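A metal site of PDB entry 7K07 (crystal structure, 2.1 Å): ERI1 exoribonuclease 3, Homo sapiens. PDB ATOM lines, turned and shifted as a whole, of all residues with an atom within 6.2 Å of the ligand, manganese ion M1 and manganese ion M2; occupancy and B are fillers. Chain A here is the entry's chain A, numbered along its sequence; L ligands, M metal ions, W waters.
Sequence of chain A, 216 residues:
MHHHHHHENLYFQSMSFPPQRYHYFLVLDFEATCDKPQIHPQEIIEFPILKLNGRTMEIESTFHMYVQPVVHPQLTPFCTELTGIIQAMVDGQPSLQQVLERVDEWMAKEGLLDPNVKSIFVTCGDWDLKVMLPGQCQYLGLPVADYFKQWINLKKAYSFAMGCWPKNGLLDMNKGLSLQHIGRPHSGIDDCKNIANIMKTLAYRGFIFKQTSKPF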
ATOM      1  N   LEU A  28       7.359  34.532  14.892  1.00  0.00           N
ATOM      2  CA  LEU A  28       6.593  33.937  15.988  1.00  0.00           C
ATOM      3  C   LEU A  28       6.127  32.549  15.589  1.00  0.00           C
ATOM      4  O   LEU A  28       5.728  32.323  14.446  1.00  0.00           O
ATOM      5  CB  LEU A  28       5.395  34.820  16.357  1.00  0.00           C
ATOM      6  CG  LEU A  28       4.460  34.352  17.467  1.00  0.00           C
ATOM      7  CD1 LEU A  28       3.965  35.554  18.228  1.00  0.00           C
ATOM      8  CD2 LEU A  28       3.284  33.567  16.903  1.00  0.00           C
ATOM      9  N   ASP A  29       6.172  31.612  16.538  1.00  0.00           N
ATOM     10  CA  ASP A  29       5.661  30.266  16.285  1.00  0.00           C
ATOM     11  C   ASP A  29       5.240  29.638  17.615  1.00  0.00           C
ATOM     12  O   ASP A  29       6.083  29.134  18.355  1.00  0.00           O
ATOM     13  CB  ASP A  29       6.695  29.398  15.591  1.00  0.00           C
ATOM     14  CG  ASP A  29       6.129  28.039  15.197  1.00  0.00           C
ATOM     15  OD1 ASP A  29       5.332  28.003  14.239  1.00  0.00           O
ATOM     16  OD2 ASP A  29       6.463  27.027  15.848  1.00  0.00           O
ATOM     17  N   PHE A  30       3.940  29.638  17.882  1.00  0.00           N
ATOM     18  CA  PHE A  30       3.428  29.013  19.088  1.00  0.00           C
ATOM     19  C   PHE A  30       3.608  27.494  19.049  1.00  0.00           C
ATOM     20  O   PHE A  30       3.586  26.879  17.986  1.00  0.00           O
ATOM     21  CB  PHE A  30       1.932  29.309  19.261  1.00  0.00           C
ATOM     22  CG  PHE A  30       1.619  30.759  19.412  1.00  0.00           C
ATOM     23  CD1 PHE A  30       2.394  31.562  20.240  1.00  0.00           C
ATOM     24  CD2 PHE A  30       0.548  31.327  18.724  1.00  0.00           C
ATOM     25  CE1 PHE A  30       2.106  32.911  20.383  1.00  0.00           C
ATOM     26  CE2 PHE A  30       0.253  32.664  18.865  1.00  0.00           C
ATOM     27  CZ  PHE A  30       1.043  33.473  19.706  1.00  0.00           C
ATOM     28  N   GLU A  31       3.816  26.910  20.236  1.00  0.00           N
ATOM     29  CA  GLU A  31       3.420  25.534  20.471  1.00  0.00           C
ATOM     30  C   GLU A  31       2.250  25.541  21.450  1.00  0.00           C
ATOM     31  O   GLU A  31       2.126  26.456  22.275  1.00  0.00           O
ATOM     32  CB  GLU A  31       4.570  24.672  21.012  1.00  0.00           C
ATOM     33  CG  GLU A  31       5.816  24.670  20.154  1.00  0.00           C
ATOM     34  CD  GLU A  31       5.580  24.177  18.719  1.00  0.00           C
ATOM     35  OE1 GLU A  31       4.700  23.311  18.507  1.00  0.00           O
ATOM     36  OE2 GLU A  31       6.289  24.668  17.814  1.00  0.00           O
ATOM     37  N   ALA A  32       1.372  24.548  21.321  1.00  0.00           N
ATOM     38  CA  ALA A  32       0.164  24.458  22.119  1.00  0.00           C
ATOM     39  C   ALA A  32      -0.013  23.042  22.641  1.00  0.00           C
ATOM     40  O   ALA A  32       0.564  22.093  22.103  1.00  0.00           O
ATOM     41  CB  ALA A  32      -1.088  24.858  21.311  1.00  0.00           C
ATOM     42  N   THR A  33      -0.804  22.917  23.705  1.00  0.00           N
ATOM     43  CA  THR A  33      -1.295  21.604  24.115  1.00  0.00           C
ATOM     44  C   THR A  33      -1.956  20.909  22.930  1.00  0.00           C
ATOM     45  O   THR A  33      -2.591  21.539  22.073  1.00  0.00           O
ATOM     46  CB  THR A  33      -2.315  21.741  25.256  1.00  0.00           C
ATOM     47  OG1 THR A  33      -3.348  22.653  24.877  1.00  0.00           O
ATOM     48  CG2 THR A  33      -1.655  22.245  26.530  1.00  0.00           C
ATOM     49  N   CYS A  34      -1.808  19.589  22.870  1.00  0.00           N
ATOM     50  CA  CYS A  34      -2.403  18.809  21.801  1.00  0.00           C
ATOM     51  C   CYS A  34      -2.601  17.377  22.291  1.00  0.00           C
ATOM     52  O   CYS A  34      -2.217  17.026  23.406  1.00  0.00           O
ATOM     53  CB  CYS A  34      -1.539  18.870  20.539  1.00  0.00           C
ATOM     54  SG  CYS A  34       0.200  18.507  20.853  1.00  0.00           S
ATOM     55  N   ASP A  35      -3.214  16.565  21.441  1.00  0.00           N
ATOM     56  CA  ASP A  35      -3.507  15.177  21.756  1.00  0.00           C
ATOM     57  C   ASP A  35      -3.996  14.504  20.472  1.00  0.00           C
ATOM     58  O   ASP A  35      -4.264  15.171  19.474  1.00  0.00           O
ATOM     59  CB  ASP A  35      -4.551  15.048  22.874  1.00  0.00           C
ATOM     60  CG  ASP A  35      -4.445  13.714  23.625  1.00  0.00           C
ATOM     61  OD1 ASP A  35      -3.626  12.858  23.227  1.00  0.00           O
ATOM     62  OD2 ASP A  35      -5.187  13.525  24.616  1.00  0.00           O
ATOM     63  N   LYS A  36      -4.092  13.183  20.519  1.00  0.00           N
ATOM     64  CA  LYS A  36      -4.664  12.368  19.443  1.00  0.00           C
ATOM     65  C   LYS A  36      -5.896  11.661  19.984  1.00  0.00           C
ATOM     66  O   LYS A  36      -5.758  10.783  20.857  1.00  0.00           O
ATOM     67  CB  LYS A  36      -3.650  11.344  18.939  1.00  0.00           C
ATOM     68  CG  LYS A  36      -3.440  11.368  17.435  1.00  0.00           C
ATOM     69  CD  LYS A  36      -2.786  12.666  16.990  1.00  0.00           C
ATOM     70  CE  LYS A  36      -2.794  12.791  15.474  1.00  0.00           C
ATOM     71  NZ  LYS A  36      -2.385  14.146  15.023  1.00  0.00           N
ATOM     72  N   GLN A  38      -7.509  15.566  18.622  1.00  0.00           N
ATOM     73  CA  GLN A  38      -7.070  16.861  19.134  1.00  0.00           C
ATOM     74  C   GLN A  38      -7.746  17.208  20.460  1.00  0.00           C
ATOM     75  O   GLN A  38      -8.918  16.898  20.682  1.00  0.00           O
ATOM     76  CB  GLN A  38      -7.339  17.954  18.101  1.00  0.00           C
ATOM     77  CG  GLN A  38      -6.577  19.255  18.363  1.00  0.00           C
ATOM     78  CD  GLN A  38      -5.081  19.043  18.634  1.00  0.00           C
ATOM     79  OE1 GLN A  38      -4.702  18.650  19.730  1.00  0.00           O
ATOM     80  NE2 GLN A  38      -4.237  19.315  17.641  1.00  0.00           N
ATOM     81  N   GLN A  42      -7.321  24.035  22.738  1.00  0.00           N
ATOM     82  CA  GLN A  42      -5.876  24.106  22.816  1.00  0.00           C
ATOM     83  C   GLN A  42      -5.459  25.359  23.575  1.00  0.00           C
ATOM     84  O   GLN A  42      -6.181  26.365  23.613  1.00  0.00           O
ATOM     85  CB  GLN A  42      -5.256  24.123  21.424  1.00  0.00           C
ATOM     86  CG  GLN A  42      -5.459  22.832  20.647  1.00  0.00           C
ATOM     87  CD  GLN A  42      -4.679  22.838  19.350  1.00  0.00           C
ATOM     88  OE1 GLN A  42      -5.197  23.239  18.316  1.00  0.00           O
ATOM     89  NE2 GLN A  42      -3.422  22.413  19.413  1.00  0.00           N
ATOM     90  N   ILE A  45       1.512  26.944  25.040  1.00  0.00           N
ATOM     91  CA  ILE A  45       2.489  26.547  26.039  1.00  0.00           C
ATOM     92  C   ILE A  45       3.890  27.047  25.740  1.00  0.00           C
ATOM     93  O   ILE A  45       4.777  26.892  26.582  1.00  0.00           O
ATOM     94  CB  ILE A  45       2.517  25.017  26.235  1.00  0.00           C
ATOM     95  CG1 ILE A  45       2.914  24.321  24.936  1.00  0.00           C
ATOM     96  CG2 ILE A  45       1.182  24.500  26.728  1.00  0.00           C
ATOM     97  CD1 ILE A  45       2.930  22.808  25.054  1.00  0.00           C
ATOM     98  N   PHE A  78       1.410  12.585  24.002  1.00  0.00           N
ATOM     99  CA  PHE A  78       1.542  12.997  22.607  1.00  0.00           C
ATOM    100  C   PHE A  78       2.156  14.384  22.504  1.00  0.00           C
ATOM    101  O   PHE A  78       3.066  14.624  21.695  1.00  0.00           O
ATOM    102  CB  PHE A  78       0.181  12.977  21.910  1.00  0.00           C
ATOM    103  CG  PHE A  78       0.245  13.458  20.508  1.00  0.00           C
ATOM    104  CD1 PHE A  78       0.598  12.598  19.481  1.00  0.00           C
ATOM    105  CD2 PHE A  78      -0.018  14.781  20.210  1.00  0.00           C
ATOM    106  CE1 PHE A  78       0.683  13.052  18.184  1.00  0.00           C
ATOM    107  CE2 PHE A  78       0.073  15.257  18.911  1.00  0.00           C
ATOM    108  CZ  PHE A  78       0.427  14.379  17.892  1.00  0.00           C
ATOM    109  N   CYS A  79       1.662  15.319  23.311  1.00  0.00           N
ATOM    110  CA  CYS A  79       2.159  16.688  23.258  1.00  0.00           C
ATOM    111  C   CYS A  79       3.650  16.747  23.567  1.00  0.00           C
ATOM    112  O   CYS A  79       4.400  17.471  22.896  1.00  0.00           O
ATOM    113  CB  CYS A  79       1.363  17.565  24.223  1.00  0.00           C
ATOM    114  SG  CYS A  79       1.920  19.265  24.327  1.00  0.00           S
ATOM    115  N   LEU A  82       5.618  15.295  20.686  1.00  0.00           N
ATOM    116  CA  LEU A  82       5.603  16.154  19.515  1.00  0.00           C
ATOM    117  C   LEU A  82       6.500  17.368  19.712  1.00  0.00           C
ATOM    118  O   LEU A  82       7.349  17.673  18.860  1.00  0.00           O
ATOM    119  CB  LEU A  82       4.171  16.596  19.205  1.00  0.00           C
ATOM    120  CG  LEU A  82       4.066  17.532  18.000  1.00  0.00           C
ATOM    121  CD1 LEU A  82       4.418  16.767  16.727  1.00  0.00           C
ATOM    122  CD2 LEU A  82       2.679  18.140  17.925  1.00  0.00           C
ATOM    123  N   THR A  83       6.343  18.077  20.837  1.00  0.00           N
ATOM    124  CA  THR A  83       7.031  19.351  21.003  1.00  0.00           C
ATOM    125  C   THR A  83       8.372  19.234  21.717  1.00  0.00           C
ATOM    126  O   THR A  83       9.200  20.145  21.605  1.00  0.00           O
ATOM    127  CB  THR A  83       6.157  20.356  21.778  1.00  0.00           C
ATOM    128  OG1 THR A  83       5.885  19.838  23.085  1.00  0.00           O
ATOM    129  CG2 THR A  83       4.822  20.612  21.030  1.00  0.00           C
ATOM    130  N   CYS A 124       4.673  30.919  10.050  1.00  0.00           N
ATOM    131  CA  CYS A 124       4.497  29.885   9.037  1.00  0.00           C
ATOM    132  C   CYS A 124       3.020  29.508   9.016  1.00  0.00           C
ATOM    133  O   CYS A 124       2.549  28.739   9.858  1.00  0.00           O
ATOM    134  CB  CYS A 124       5.385  28.683   9.336  1.00  0.00           C
ATOM    135  SG  CYS A 124       5.348  27.423   8.004  1.00  0.00           S
ATOM    136  N   TRP A 127      -2.306  30.162  11.157  1.00  0.00           N
ATOM    137  CA  TRP A 127      -2.957  29.590  12.333  1.00  0.00           C
ATOM    138  C   TRP A 127      -2.621  30.352  13.618  1.00  0.00           C
ATOM    139  O   TRP A 127      -3.512  30.607  14.445  1.00  0.00           O
ATOM    140  CB  TRP A 127      -2.566  28.111  12.467  1.00  0.00           C
ATOM    141  CG  TRP A 127      -3.097  27.436  13.688  1.00  0.00           C
ATOM    142  CD1 TRP A 127      -4.368  26.949  13.877  1.00  0.00           C
ATOM    143  CD2 TRP A 127      -2.387  27.188  14.904  1.00  0.00           C
ATOM    144  NE1 TRP A 127      -4.478  26.410  15.136  1.00  0.00           N
ATOM    145  CE2 TRP A 127      -3.281  26.540  15.785  1.00  0.00           C
ATOM    146  CE3 TRP A 127      -1.070  27.449  15.342  1.00  0.00           C
ATOM    147  CZ2 TRP A 127      -2.901  26.133  17.066  1.00  0.00           C
ATOM    148  CZ3 TRP A 127      -0.705  27.045  16.606  1.00  0.00           C
ATOM    149  CH2 TRP A 127      -1.622  26.405  17.460  1.00  0.00           C
ATOM    150  N   ASP A 128      -1.357  30.745  13.800  1.00  0.00           N
ATOM    151  CA  ASP A 128      -0.927  31.313  15.079  1.00  0.00           C
ATOM    152  C   ASP A 128      -1.736  32.538  15.462  1.00  0.00           C
ATOM    153  O   ASP A 128      -2.281  32.624  16.563  1.00  0.00           O
ATOM    154  CB  ASP A 128       0.571  31.665  15.042  1.00  0.00           C
ATOM    155  CG  ASP A 128       1.428  30.494  14.672  1.00  0.00           C
ATOM    156  OD1 ASP A 128       2.104  29.941  15.571  1.00  0.00           O
ATOM    157  OD2 ASP A 128       1.390  30.093  13.479  1.00  0.00           O
ATOM    158  N   HIS A 186       9.308  21.043  15.422  1.00  0.00           N
ATOM    159  CA  HIS A 186       8.205  21.232  16.354  1.00  0.00           C
ATOM    160  C   HIS A 186       8.660  21.791  17.707  1.00  0.00           C
ATOM    161  O   HIS A 186       7.922  21.681  18.701  1.00  0.00           O
ATOM    162  CB  HIS A 186       7.420  19.930  16.546  1.00  0.00           C
ATOM    163  CG  HIS A 186       7.028  19.289  15.245  1.00  0.00           C
ATOM    164  ND1 HIS A 186       5.915  19.674  14.527  1.00  0.00           N
ATOM    165  CD2 HIS A 186       7.627  18.306  14.536  1.00  0.00           C
ATOM    166  CE1 HIS A 186       5.833  18.950  13.430  1.00  0.00           C
ATOM    167  NE2 HIS A 186       6.858  18.113  13.401  1.00  0.00           N
ATOM    168  N   SER A 187       9.838  22.387  17.766  1.00  0.00           N
ATOM    169  CA  SER A 187      10.200  23.297  18.841  1.00  0.00           C
ATOM    170  C   SER A 187       9.876  24.709  18.386  1.00  0.00           C
ATOM    171  O   SER A 187      10.269  25.122  17.289  1.00  0.00           O
ATOM    172  CB  SER A 187      11.687  23.189  19.197  1.00  0.00           C
ATOM    173  OG  SER A 187      12.086  24.281  20.015  1.00  0.00           O
ATOM    174  N   GLY A 188       9.146  25.448  19.235  1.00  0.00           N
ATOM    175  CA  GLY A 188       8.736  26.792  18.836  1.00  0.00           C
ATOM    176  C   GLY A 188       9.910  27.686  18.491  1.00  0.00           C
ATOM    177  O   GLY A 188       9.932  28.323  17.431  1.00  0.00           O
ATOM    178  N   ASP A 191      11.599  26.425  15.277  1.00  0.00           N
ATOM    179  CA  ASP A 191      10.807  26.799  14.105  1.00  0.00           C
ATOM    180  C   ASP A 191      11.024  28.264  13.755  1.00  0.00           C
ATOM    181  O   ASP A 191      11.154  28.620  12.574  1.00  0.00           O
ATOM    182  CB  ASP A 191       9.323  26.497  14.345  1.00  0.00           C
ATOM    183  CG  ASP A 191       9.022  25.000  14.353  1.00  0.00           C
ATOM    184  OD1 ASP A 191       9.854  24.221  13.833  1.00  0.00           O
ATOM    185  OD2 ASP A 191       7.952  24.599  14.865  1.00  0.00           O
HETATM  186  P1  LIG L   1       3.337  23.817  14.252  1.00  0.00           P
HETATM  187  O1  LIG L   1       2.261  24.572  13.517  1.00  0.00           O
HETATM  188  O2  LIG L   1       4.467  24.715  14.709  1.00  0.00           O
HETATM  189  O3  LIG L   1       3.832  22.557  13.603  1.00  0.00           O
HETATM  190  O4  LIG L   1       2.618  23.313  15.584  1.00  0.00           O
HETATM  191  C1  LIG L   1       1.680  24.122  16.280  1.00  0.00           C
HETATM  192  C2  LIG L   1       0.818  23.303  17.215  1.00  0.00           C
HETATM  193  O5  LIG L   1      -0.170  22.556  16.444  1.00  0.00           O
HETATM  194  C3  LIG L   1       1.524  22.236  18.048  1.00  0.00           C
HETATM  195  O6  LIG L   1       2.143  22.768  19.223  1.00  0.00           O
HETATM  196  C4  LIG L   1       0.416  21.243  18.337  1.00  0.00           C
HETATM  197  O7  LIG L   1      -0.413  21.714  19.382  1.00  0.00           O
HETATM  198  C5  LIG L   1      -0.379  21.286  17.023  1.00  0.00           C
HETATM  199  N1  LIG L   1       0.113  20.266  16.083  1.00  0.00           N
HETATM  200  C6  LIG L   1       1.130  20.422  15.195  1.00  0.00           C
HETATM  201  N2  LIG L   1       1.356  19.270  14.509  1.00  0.00           N
HETATM  202  C7  LIG L   1       0.471  18.363  14.948  1.00  0.00           C
HETATM  203  C8  LIG L   1       0.166  16.949  14.636  1.00  0.00           C
HETATM  204  N3  LIG L   1       0.874  16.294  13.687  1.00  0.00           N
HETATM  205  N4  LIG L   1      -0.816  16.358  15.344  1.00  0.00           N
HETATM  206  C9  LIG L   1      -1.523  17.014  16.293  1.00  0.00           C
HETATM  207  N5  LIG L   1      -1.311  18.296  16.621  1.00  0.00           N
HETATM  208  C10 LIG L   1      -0.332  19.013  15.996  1.00  0.00           C
HETATM  209 MN    MN M   1       6.188  24.904  15.741  1.00  0.00          MN
HETATM  210 MN    MN M   2       3.732  26.648  13.700  1.00  0.00          MN
HETATM  211  O   HOH W   1       2.664  27.322  15.506  1.00  0.00           O
HETATM  212  O   HOH W   2      -3.453  22.647  16.014  1.00  0.00           O
HETATM  213  O   HOH W   3       5.516  22.713  16.023  1.00  0.00           O
HETATM  214  O   HOH W   4       5.518  25.863  12.142  1.00  0.00           O
HETATM  215  O   HOH W   5       2.521  28.201  12.706  1.00  0.00           O
HETATM  216  O   HOH W   6       3.019  22.202  11.101  1.00  0.00           O
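N of Asp 35 sits at hydrogen-bond distance from OE1 of Gln 38, at 3.1 Å.
O of Glu 31 sits at hydrogen-bond distance from N of Ile 45, at 2.9 Å.
OD1 of Asp 128 sits at hydrogen-bond distance from N of Phe 30 (3.0 Å).
The backbone NH (N) of Gly 188 lies close to the side-chain carboxylate (OE2) of Glu 31, 3.3 Å away.
The side-chain hydroxyl (OG1) of Thr 83 lies within hydrogen-bond range of the backbone carbonyl oxygen (O) of Cys 79, 2.8 Å away.
The side-chain amide nitrogen (NE2) of Gln 42 is in hydrogen-bond range of the backbone carbonyl oxygen (O) of Thr 33, 2.9 Å away.
Residues that only touch the ligand: Phe 30, Phe 78, Leu 82, Thr 83, Trp 127 and His 186.
Of the 23 residues printed, 15 come within 4 Å of the ligand.
The nearest printed residue that does not touch the ligand is Asp 35 (4.6 Å).
Manganese ion M1 is bound by OD2 of Asp 191, O2 of the ligand, OE2 of Glu 31, OD2 of Asp 29 and water W3.
Water W3 lies within hydrogen-bond range of OE1 of Glu 31, O3 of the ligand and ND1 of His 186.
Water W1 bridges the side-chain carboxylate of Asp 128 (2.7 Å) and the backbone carbonyl oxygen of Phe 30 (2.7 Å).
Water W5 bridges O of Cys 124 (2.9 Å) and OD1 of Asp 128 (3.4 Å).
Water W2 bridges the side-chain amide oxygen (OE1) of Gln 42 (2.9 Å) and an oxygen (O5) of the ligand (3.3 Å).
Phe 30 touches manganese ion M1 (O to MN, 3.96 Å).
Within 4 Å of manganese ion M1: Asp 29, Phe 30, Glu 31 and Asp 191.
N5 of the ligand sits at hydrogen-bond distance from NE2 of Gln 38.
The side-chain sulfur (SG) of Cys 34 lies close to an oxygen (O7) of the ligand (3.6 Å).
O of Thr 33 is in hydrogen-bond range of O7 of the ligand (3.5 Å).
An oxygen (O6) of the ligand lies within hydrogen-bond range of the backbone NH of Ala 32.
The backbone carbonyl oxygen (O) of Ala 32 lies within hydrogen-bond range of an oxygen (O7) of the ligand (2.9 Å).
NE2 of Gln 42 lies within hydrogen-bond range of O7 of the ligand (3.1 Å).
The side-chain amino group of Lys 36 lies within hydrogen-bond range of a nitrogen (N4) of the ligand (2.7 Å).
Manganese ion M2 is bound by OD1 of Asp 29 (2.2 Å).
Manganese ion M2 is bound by water W1, 2.2 Å away.
Manganese ion M2 is bound by water W5 (2.2 Å).
An oxygen (O2) of the ligand binds manganese ion M2 (2.3 Å).
Water W4 binds manganese ion M2 (2.5 Å).
O1 of the ligand binds manganese ion M2 (2.6 Å).
Within 4 Å of manganese ion M2: Asp 29.
The nearest printed residue that does not touch manganese ion M2 is Asp 128 (4.1 Å).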
